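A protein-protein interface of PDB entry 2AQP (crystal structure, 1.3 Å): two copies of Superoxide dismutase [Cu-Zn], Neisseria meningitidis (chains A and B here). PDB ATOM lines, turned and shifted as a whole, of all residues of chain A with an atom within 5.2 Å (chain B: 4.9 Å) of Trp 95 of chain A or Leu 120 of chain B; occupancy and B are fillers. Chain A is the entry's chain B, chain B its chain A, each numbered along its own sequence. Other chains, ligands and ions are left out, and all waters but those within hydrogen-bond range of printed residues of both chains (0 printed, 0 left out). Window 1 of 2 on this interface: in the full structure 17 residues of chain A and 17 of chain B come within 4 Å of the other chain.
Leu 120 of chain A touches Pro 122 of chain B, and with the chains exchanged Pro 122 of chain A touches Leu 120 of chain B. Of the 10 pairs that touch across the chains among the printed residues, 2 have their exchanged pair printed and touching as well.
Tyr 93 of chain A touches none of the printed residues of chain B. Of chain B, only Ser 36 (3.9 Å), Tyr 38 (3.4 Å), Val 41 (3.6 Å), Pro 118 (3.8 Å) and Leu 120 (3.7 Å) come within 4 Å of Trp 95 of chain A. Gln 96 of chain A touches none of the printed residues of chain B. Of the printed residues of chain B, Pro 122 of chain A touches Tyr 38 (3.7 Å) and Leu 120 (3.7 Å). Printed residues of chain A within 4 Å of Tyr 38 of chain B: Trp 95, Asp 97, Pro 122 and Arg 123. Printed residues of chain A within 4 Å of Pro 118 of chain B: Trp 95 (3.8 Å). Printed residues of chain A within 4 Å of Pro 122 of chain B: Leu 120 (3.6 Å). The nearest residue of chain A that does not touch Leu 120 of chain B is Leu 120 of chain A (4.5 Å). The nearest printed residue of chain A that does not touch Tyr 38 of chain B is Gln 96 of chain A (4.9 Å).
OG of Ser 36 of chain B lies within hydrogen-bond range of N of Tyr 38 of chain B, at 3.0 Å. OG of Ser 36 of chain B sits at hydrogen-bond distance from O of Gly 39 of chain B, 2.8 Å away. NH2 of Arg 123 of chain A lies within hydrogen-bond range of O of Tyr 93 of chain A (3.1 Å). The backbone carbonyl oxygen (O) of Pro 94 of chain A is in hydrogen-bond range of the guanidinium group (NE) of Arg 123 of chain A, 2.9 Å away. The backbone carbonyl oxygen (O) of Gln 96 of chain A lies close to the guanidinium group (NE) of Arg 123 of chain A.
Hydrophobic or aromatic side chains of chain A within 4 Å of the printed part of chain B: Trp 95, Leu 120 and Pro 122. Of the 12 printed residues of chain B, 6 touch a printed residue of chain A. Hydrophobic or aromatic side chains of chain B that line the printed part of chain A: Tyr 38, Val 41, Pro 118, Leu 120 and Pro 122. Among the printed residues, no Asp or Glu carboxylate lies within 4 Å of a Lys or Arg side-chain nitrogen of the other chain.
The side-chain carboxylate (OD1) of Asp 97 of chain A sits at hydrogen-bond distance from the side-chain hydroxyl (OH) of Tyr 38 of chain B (2.5 Å).
OG of Ser 36 of chain B touches CB of Trp 95 of chain A, 3.9 Å away. O of Trp 95 of chain A touches CD2 of Tyr 38 of chain B, at 3.4 Å. Val 41 of chain B touches Trp 95 of chain A. Pro 118 of chain B touches Trp 95 of chain A (CG to CZ2, 3.8 Å). Leu 120 of chain B touches Trp 95 of chain A (CB to CE3, 3.7 Å). CD2 of Leu 120 of chain A touches CG of Pro 122 of chain B, at 3.6 Å. Pro 122 of chain A touches Tyr 38 of chain B. Pro 122 of chain A touches Leu 120 of chain B (CG to CD2, 3.7 Å). Tyr 38 of chain B touches Arg 123 of chain A.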
ATOM      1  N   TYR A  93     -29.835  16.798 -27.607  1.00  0.00           N
ATOM      2  CA  TYR A  93     -28.677  17.232 -26.869  1.00  0.00           C
ATOM      3  C   TYR A  93     -28.488  18.740 -26.810  1.00  0.00           C
ATOM      4  O   TYR A  93     -28.976  19.462 -27.672  1.00  0.00           O
ATOM      5  CB  TYR A  93     -27.395  16.623 -27.478  1.00  0.00           C
ATOM      6  CG  TYR A  93     -27.301  15.116 -27.325  1.00  0.00           C
ATOM      7  CD1 TYR A  93     -26.813  14.549 -26.147  1.00  0.00           C
ATOM      8  CD2 TYR A  93     -27.704  14.293 -28.365  1.00  0.00           C
ATOM      9  CE1 TYR A  93     -26.733  13.187 -26.036  1.00  0.00           C
ATOM     10  CE2 TYR A  93     -27.633  12.923 -28.248  1.00  0.00           C
ATOM     11  CZ  TYR A  93     -27.144  12.390 -27.078  1.00  0.00           C
ATOM     12  OH  TYR A  93     -27.079  11.023 -26.958  1.00  0.00           O
ATOM     13  N   PRO A  94     -27.787  19.227 -25.797  1.00  0.00           N
ATOM     14  CA  PRO A  94     -27.522  20.651 -25.760  1.00  0.00           C
ATOM     15  C   PRO A  94     -26.730  21.172 -26.964  1.00  0.00           C
ATOM     16  O   PRO A  94     -26.857  22.373 -27.279  1.00  0.00           O
ATOM     17  CB  PRO A  94     -26.758  20.840 -24.436  1.00  0.00           C
ATOM     18  CG  PRO A  94     -27.168  19.664 -23.595  1.00  0.00           C
ATOM     19  CD  PRO A  94     -27.263  18.552 -24.602  1.00  0.00           C
ATOM     20  N   TRP A  95     -25.936  20.271 -27.573  1.00  0.00           N
ATOM     21  CA  TRP A  95     -25.094  20.603 -28.696  1.00  0.00           C
ATOM     22  C   TRP A  95     -25.657  20.137 -30.048  1.00  0.00           C
ATOM     23  O   TRP A  95     -24.985  20.120 -31.067  1.00  0.00           O
ATOM     24  CB  TRP A  95     -23.685  20.037 -28.471  1.00  0.00           C
ATOM     25  CG  TRP A  95     -23.752  18.650 -27.894  1.00  0.00           C
ATOM     26  CD1 TRP A  95     -23.877  17.467 -28.564  1.00  0.00           C
ATOM     27  CD2 TRP A  95     -23.726  18.297 -26.507  1.00  0.00           C
ATOM     28  NE1 TRP A  95     -23.912  16.404 -27.672  1.00  0.00           N
ATOM     29  CE2 TRP A  95     -23.819  16.891 -26.415  1.00  0.00           C
ATOM     30  CE3 TRP A  95     -23.609  19.047 -25.331  1.00  0.00           C
ATOM     31  CZ2 TRP A  95     -23.811  16.200 -25.210  1.00  0.00           C
ATOM     32  CZ3 TRP A  95     -23.606  18.353 -24.109  1.00  0.00           C
ATOM     33  CH2 TRP A  95     -23.711  16.962 -24.088  1.00  0.00           C
ATOM     34  N   GLN A  96     -26.960  19.820 -30.063  1.00  0.00           N
ATOM     35  CA  GLN A  96     -27.666  19.345 -31.244  1.00  0.00           C
ATOM     36  C   GLN A  96     -28.523  20.431 -31.861  1.00  0.00           C
ATOM     37  O   GLN A  96     -29.475  20.910 -31.253  1.00  0.00           O
ATOM     38  CB  GLN A  96     -28.548  18.174 -30.820  1.00  0.00           C
ATOM     39  CG  GLN A  96     -29.337  17.568 -31.973  1.00  0.00           C
ATOM     40  CD  GLN A  96     -30.188  16.407 -31.543  1.00  0.00           C
ATOM     41  OE1 GLN A  96     -30.011  15.864 -30.447  1.00  0.00           O
ATOM     42  NE2 GLN A  96     -31.157  15.960 -32.340  1.00  0.00           N
ATOM     43  N   ASP A  97     -28.168  20.796 -33.107  1.00  0.00           N
ATOM     44  CA  ASP A  97     -28.862  21.918 -33.693  1.00  0.00           C
ATOM     45  C   ASP A  97     -30.308  21.611 -34.059  1.00  0.00           C
ATOM     46  O   ASP A  97     -31.066  22.582 -34.092  1.00  0.00           O
ATOM     47  CB  ASP A  97     -28.076  22.382 -34.941  1.00  0.00           C
ATOM     48  CG  ASP A  97     -26.832  23.144 -34.540  1.00  0.00           C
ATOM     49  OD1 ASP A  97     -26.866  23.806 -33.495  1.00  0.00           O
ATOM     50  OD2 ASP A  97     -25.868  23.096 -35.339  1.00  0.00           O
ATOM     51  N   PRO A 105     -27.993  21.077 -20.585  1.00  0.00           N
ATOM     52  CA  PRO A 105     -27.395  19.943 -19.885  1.00  0.00           C
ATOM     53  C   PRO A 105     -28.164  19.639 -18.589  1.00  0.00           C
ATOM     54  O   PRO A 105     -28.712  20.542 -17.980  1.00  0.00           O
ATOM     55  CB  PRO A 105     -25.959  20.398 -19.599  1.00  0.00           C
ATOM     56  CG  PRO A 105     -25.692  21.506 -20.581  1.00  0.00           C
ATOM     57  CD  PRO A 105     -27.038  22.180 -20.706  1.00  0.00           C
ATOM     58  N   LEU A 120     -23.220  24.706 -19.330  1.00  0.00           N
ATOM     59  CA  LEU A 120     -23.214  25.555 -20.533  1.00  0.00           C
ATOM     60  C   LEU A 120     -24.224  25.099 -21.560  1.00  0.00           C
ATOM     61  O   LEU A 120     -24.332  23.911 -21.903  1.00  0.00           O
ATOM     62  CB  LEU A 120     -21.804  25.462 -21.136  1.00  0.00           C
ATOM     63  CG  LEU A 120     -21.634  26.149 -22.493  1.00  0.00           C
ATOM     64  CD1 LEU A 120     -21.648  27.674 -22.402  1.00  0.00           C
ATOM     65  CD2 LEU A 120     -20.313  25.703 -23.140  1.00  0.00           C
ATOM     66  N   PRO A 122     -24.484  25.795 -25.291  1.00  0.00           N
ATOM     67  CA  PRO A 122     -23.724  26.467 -26.354  1.00  0.00           C
ATOM     68  C   PRO A 122     -24.605  27.031 -27.440  1.00  0.00           C
ATOM     69  O   PRO A 122     -24.112  27.927 -28.168  1.00  0.00           O
ATOM     70  CB  PRO A 122     -22.823  25.344 -26.900  1.00  0.00           C
ATOM     71  CG  PRO A 122     -23.657  24.107 -26.633  1.00  0.00           C
ATOM     72  CD  PRO A 122     -24.219  24.359 -25.245  1.00  0.00           C
ATOM     73  N   ARG A 123     -25.835  26.577 -27.582  1.00  0.00           N
ATOM     74  CA  ARG A 123     -26.678  27.177 -28.636  1.00  0.00           C
ATOM     75  C   ARG A 123     -27.388  28.442 -28.240  1.00  0.00           C
ATOM     76  O   ARG A 123     -28.048  29.069 -29.053  1.00  0.00           O
ATOM     77  CB  ARG A 123     -27.716  26.140 -29.070  1.00  0.00           C
ATOM     78  CG  ARG A 123     -27.048  24.952 -29.716  1.00  0.00           C
ATOM     79  CD  ARG A 123     -27.999  23.924 -30.245  1.00  0.00           C
ATOM     80  NE  ARG A 123     -28.793  23.158 -29.323  1.00  0.00           N
ATOM     81  CZ  ARG A 123     -30.088  22.904 -29.259  1.00  0.00           C
ATOM     82  NH1 ARG A 123     -30.953  23.451 -30.143  1.00  0.00           N
ATOM     83  NH2 ARG A 123     -30.522  22.102 -28.270  1.00  0.00           N
ATOM     84  N   SER B  36     -18.649  17.484 -31.921  1.00  0.00           N
ATOM     85  CA  SER B  36     -19.907  18.159 -32.196  1.00  0.00           C
ATOM     86  C   SER B  36     -19.590  19.522 -32.816  1.00  0.00           C
ATOM     87  O   SER B  36     -18.462  20.017 -32.750  1.00  0.00           O
ATOM     88  CB  SER B  36     -20.728  18.355 -30.922  1.00  0.00           C
ATOM     89  OG  SER B  36     -20.304  19.513 -30.242  1.00  0.00           O
ATOM     90  N   TYR B  38     -20.022  22.182 -31.535  1.00  0.00           N
ATOM     91  CA  TYR B  38     -19.730  23.091 -30.444  1.00  0.00           C
ATOM     92  C   TYR B  38     -18.488  22.658 -29.682  1.00  0.00           C
ATOM     93  O   TYR B  38     -18.151  23.300 -28.679  1.00  0.00           O
ATOM     94  CB  TYR B  38     -20.936  23.239 -29.469  1.00  0.00           C
ATOM     95  CG  TYR B  38     -22.090  23.765 -30.322  1.00  0.00           C
ATOM     96  CD1 TYR B  38     -22.137  25.134 -30.541  1.00  0.00           C
ATOM     97  CD2 TYR B  38     -23.019  22.942 -30.894  1.00  0.00           C
ATOM     98  CE1 TYR B  38     -23.183  25.664 -31.338  1.00  0.00           C
ATOM     99  CE2 TYR B  38     -24.056  23.437 -31.713  1.00  0.00           C
ATOM    100  CZ  TYR B  38     -24.093  24.816 -31.904  1.00  0.00           C
ATOM    101  OH  TYR B  38     -25.081  25.404 -32.698  1.00  0.00           O
ATOM    102  N   GLY B  39     -17.814  21.586 -30.105  1.00  0.00           N
ATOM    103  CA  GLY B  39     -16.620  21.081 -29.431  1.00  0.00           C
ATOM    104  C   GLY B  39     -16.696  19.610 -29.134  1.00  0.00           C
ATOM    105  O   GLY B  39     -17.677  18.938 -29.474  1.00  0.00           O
ATOM    106  N   LEU B  40     -15.711  19.046 -28.413  1.00  0.00           N
ATOM    107  CA  LEU B  40     -15.669  17.621 -28.161  1.00  0.00           C
ATOM    108  C   LEU B  40     -16.650  17.226 -27.058  1.00  0.00           C
ATOM    109  O   LEU B  40     -16.743  17.910 -26.038  1.00  0.00           O
ATOM    110  CB  LEU B  40     -14.254  17.137 -27.749  1.00  0.00           C
ATOM    111  CG  LEU B  40     -13.177  17.309 -28.822  1.00  0.00           C
ATOM    112  CD1 LEU B  40     -11.922  16.570 -28.358  1.00  0.00           C
ATOM    113  CD2 LEU B  40     -13.603  16.811 -30.198  1.00  0.00           C
ATOM    114  N   VAL B  41     -17.338  16.123 -27.299  1.00  0.00           N
ATOM    115  CA  VAL B  41     -18.282  15.544 -26.383  1.00  0.00           C
ATOM    116  C   VAL B  41     -17.679  14.263 -25.797  1.00  0.00           C
ATOM    117  O   VAL B  41     -17.154  13.397 -26.525  1.00  0.00           O
ATOM    118  CB  VAL B  41     -19.635  15.270 -27.069  1.00  0.00           C
ATOM    119  CG1 VAL B  41     -20.564  14.545 -26.078  1.00  0.00           C
ATOM    120  CG2 VAL B  41     -20.296  16.556 -27.551  1.00  0.00           C
ATOM    121  N   PRO B  94     -14.688  25.075 -18.001  1.00  0.00           N
ATOM    122  CA  PRO B  94     -14.572  24.551 -19.366  1.00  0.00           C
ATOM    123  C   PRO B  94     -14.702  25.603 -20.446  1.00  0.00           C
ATOM    124  O   PRO B  94     -14.192  25.413 -21.566  1.00  0.00           O
ATOM    125  CB  PRO B  94     -15.722  23.511 -19.423  1.00  0.00           C
ATOM    126  CG  PRO B  94     -15.968  23.115 -18.004  1.00  0.00           C
ATOM    127  CD  PRO B  94     -15.775  24.414 -17.262  1.00  0.00           C
ATOM    128  N   PRO B 105     -15.979  19.709 -18.048  1.00  0.00           N
ATOM    129  CA  PRO B 105     -17.061  19.691 -17.069  1.00  0.00           C
ATOM    130  C   PRO B 105     -16.939  18.485 -16.152  1.00  0.00           C
ATOM    131  O   PRO B 105     -16.446  17.459 -16.535  1.00  0.00           O
ATOM    132  CB  PRO B 105     -18.343  19.647 -17.908  1.00  0.00           C
ATOM    133  CG  PRO B 105     -17.897  20.134 -19.267  1.00  0.00           C
ATOM    134  CD  PRO B 105     -16.488  19.628 -19.419  1.00  0.00           C
ATOM    135  N   PRO B 118     -23.279  12.664 -20.793  1.00  0.00           N
ATOM    136  CA  PRO B 118     -22.201  13.249 -21.562  1.00  0.00           C
ATOM    137  C   PRO B 118     -21.957  14.725 -21.186  1.00  0.00           C
ATOM    138  O   PRO B 118     -22.893  15.393 -20.695  1.00  0.00           O
ATOM    139  CB  PRO B 118     -22.710  13.176 -23.017  1.00  0.00           C
ATOM    140  CG  PRO B 118     -24.211  13.271 -22.850  1.00  0.00           C
ATOM    141  CD  PRO B 118     -24.535  12.556 -21.555  1.00  0.00           C
ATOM    142  N   VAL B 119     -20.734  15.172 -21.471  1.00  0.00           N
ATOM    143  CA  VAL B 119     -20.378  16.553 -21.203  1.00  0.00           C
ATOM    144  C   VAL B 119     -19.587  17.106 -22.393  1.00  0.00           C
ATOM    145  O   VAL B 119     -18.865  16.388 -23.082  1.00  0.00           O
ATOM    146  CB  VAL B 119     -19.592  16.746 -19.906  1.00  0.00           C
ATOM    147  CG1 VAL B 119     -20.373  16.286 -18.683  1.00  0.00           C
ATOM    148  CG2 VAL B 119     -18.240  16.043 -19.962  1.00  0.00           C
ATOM    149  N   LEU B 120     -19.766  18.395 -22.633  1.00  0.00           N
ATOM    150  CA  LEU B 120     -19.131  19.106 -23.757  1.00  0.00           C
ATOM    151  C   LEU B 120     -17.970  19.941 -23.272  1.00  0.00           C
ATOM    152  O   LEU B 120     -18.040  20.693 -22.291  1.00  0.00           O
ATOM    153  CB  LEU B 120     -20.159  20.069 -24.342  1.00  0.00           C
ATOM    154  CG  LEU B 120     -19.678  21.002 -25.444  1.00  0.00           C
ATOM    155  CD1 LEU B 120     -19.294  20.257 -26.723  1.00  0.00           C
ATOM    156  CD2 LEU B 120     -20.771  22.009 -25.752  1.00  0.00           C
ATOM    157  N   ALA B 121     -16.850  19.861 -23.996  1.00  0.00           N
ATOM    158  CA  ALA B 121     -15.690  20.692 -23.806  1.00  0.00           C
ATOM    159  C   ALA B 121     -15.585  21.693 -24.961  1.00  0.00           C
ATOM    160  O   ALA B 121     -15.017  21.347 -26.024  1.00  0.00           O
ATOM    161  CB  ALA B 121     -14.400  19.898 -23.693  1.00  0.00           C
ATOM    162  N   PRO B 122     -16.162  22.885 -24.863  1.00  0.00           N
ATOM    163  CA  PRO B 122     -16.277  23.761 -26.031  1.00  0.00           C
ATOM    164  C   PRO B 122     -14.954  24.297 -26.533  1.00  0.00           C
ATOM    165  O   PRO B 122     -14.897  24.710 -27.723  1.00  0.00           O
ATOM    166  CB  PRO B 122     -17.181  24.915 -25.545  1.00  0.00           C
ATOM    167  CG  PRO B 122     -16.869  24.965 -24.060  1.00  0.00           C
ATOM    168  CD  PRO B 122     -16.772  23.495 -23.665  1.00  0.00           C
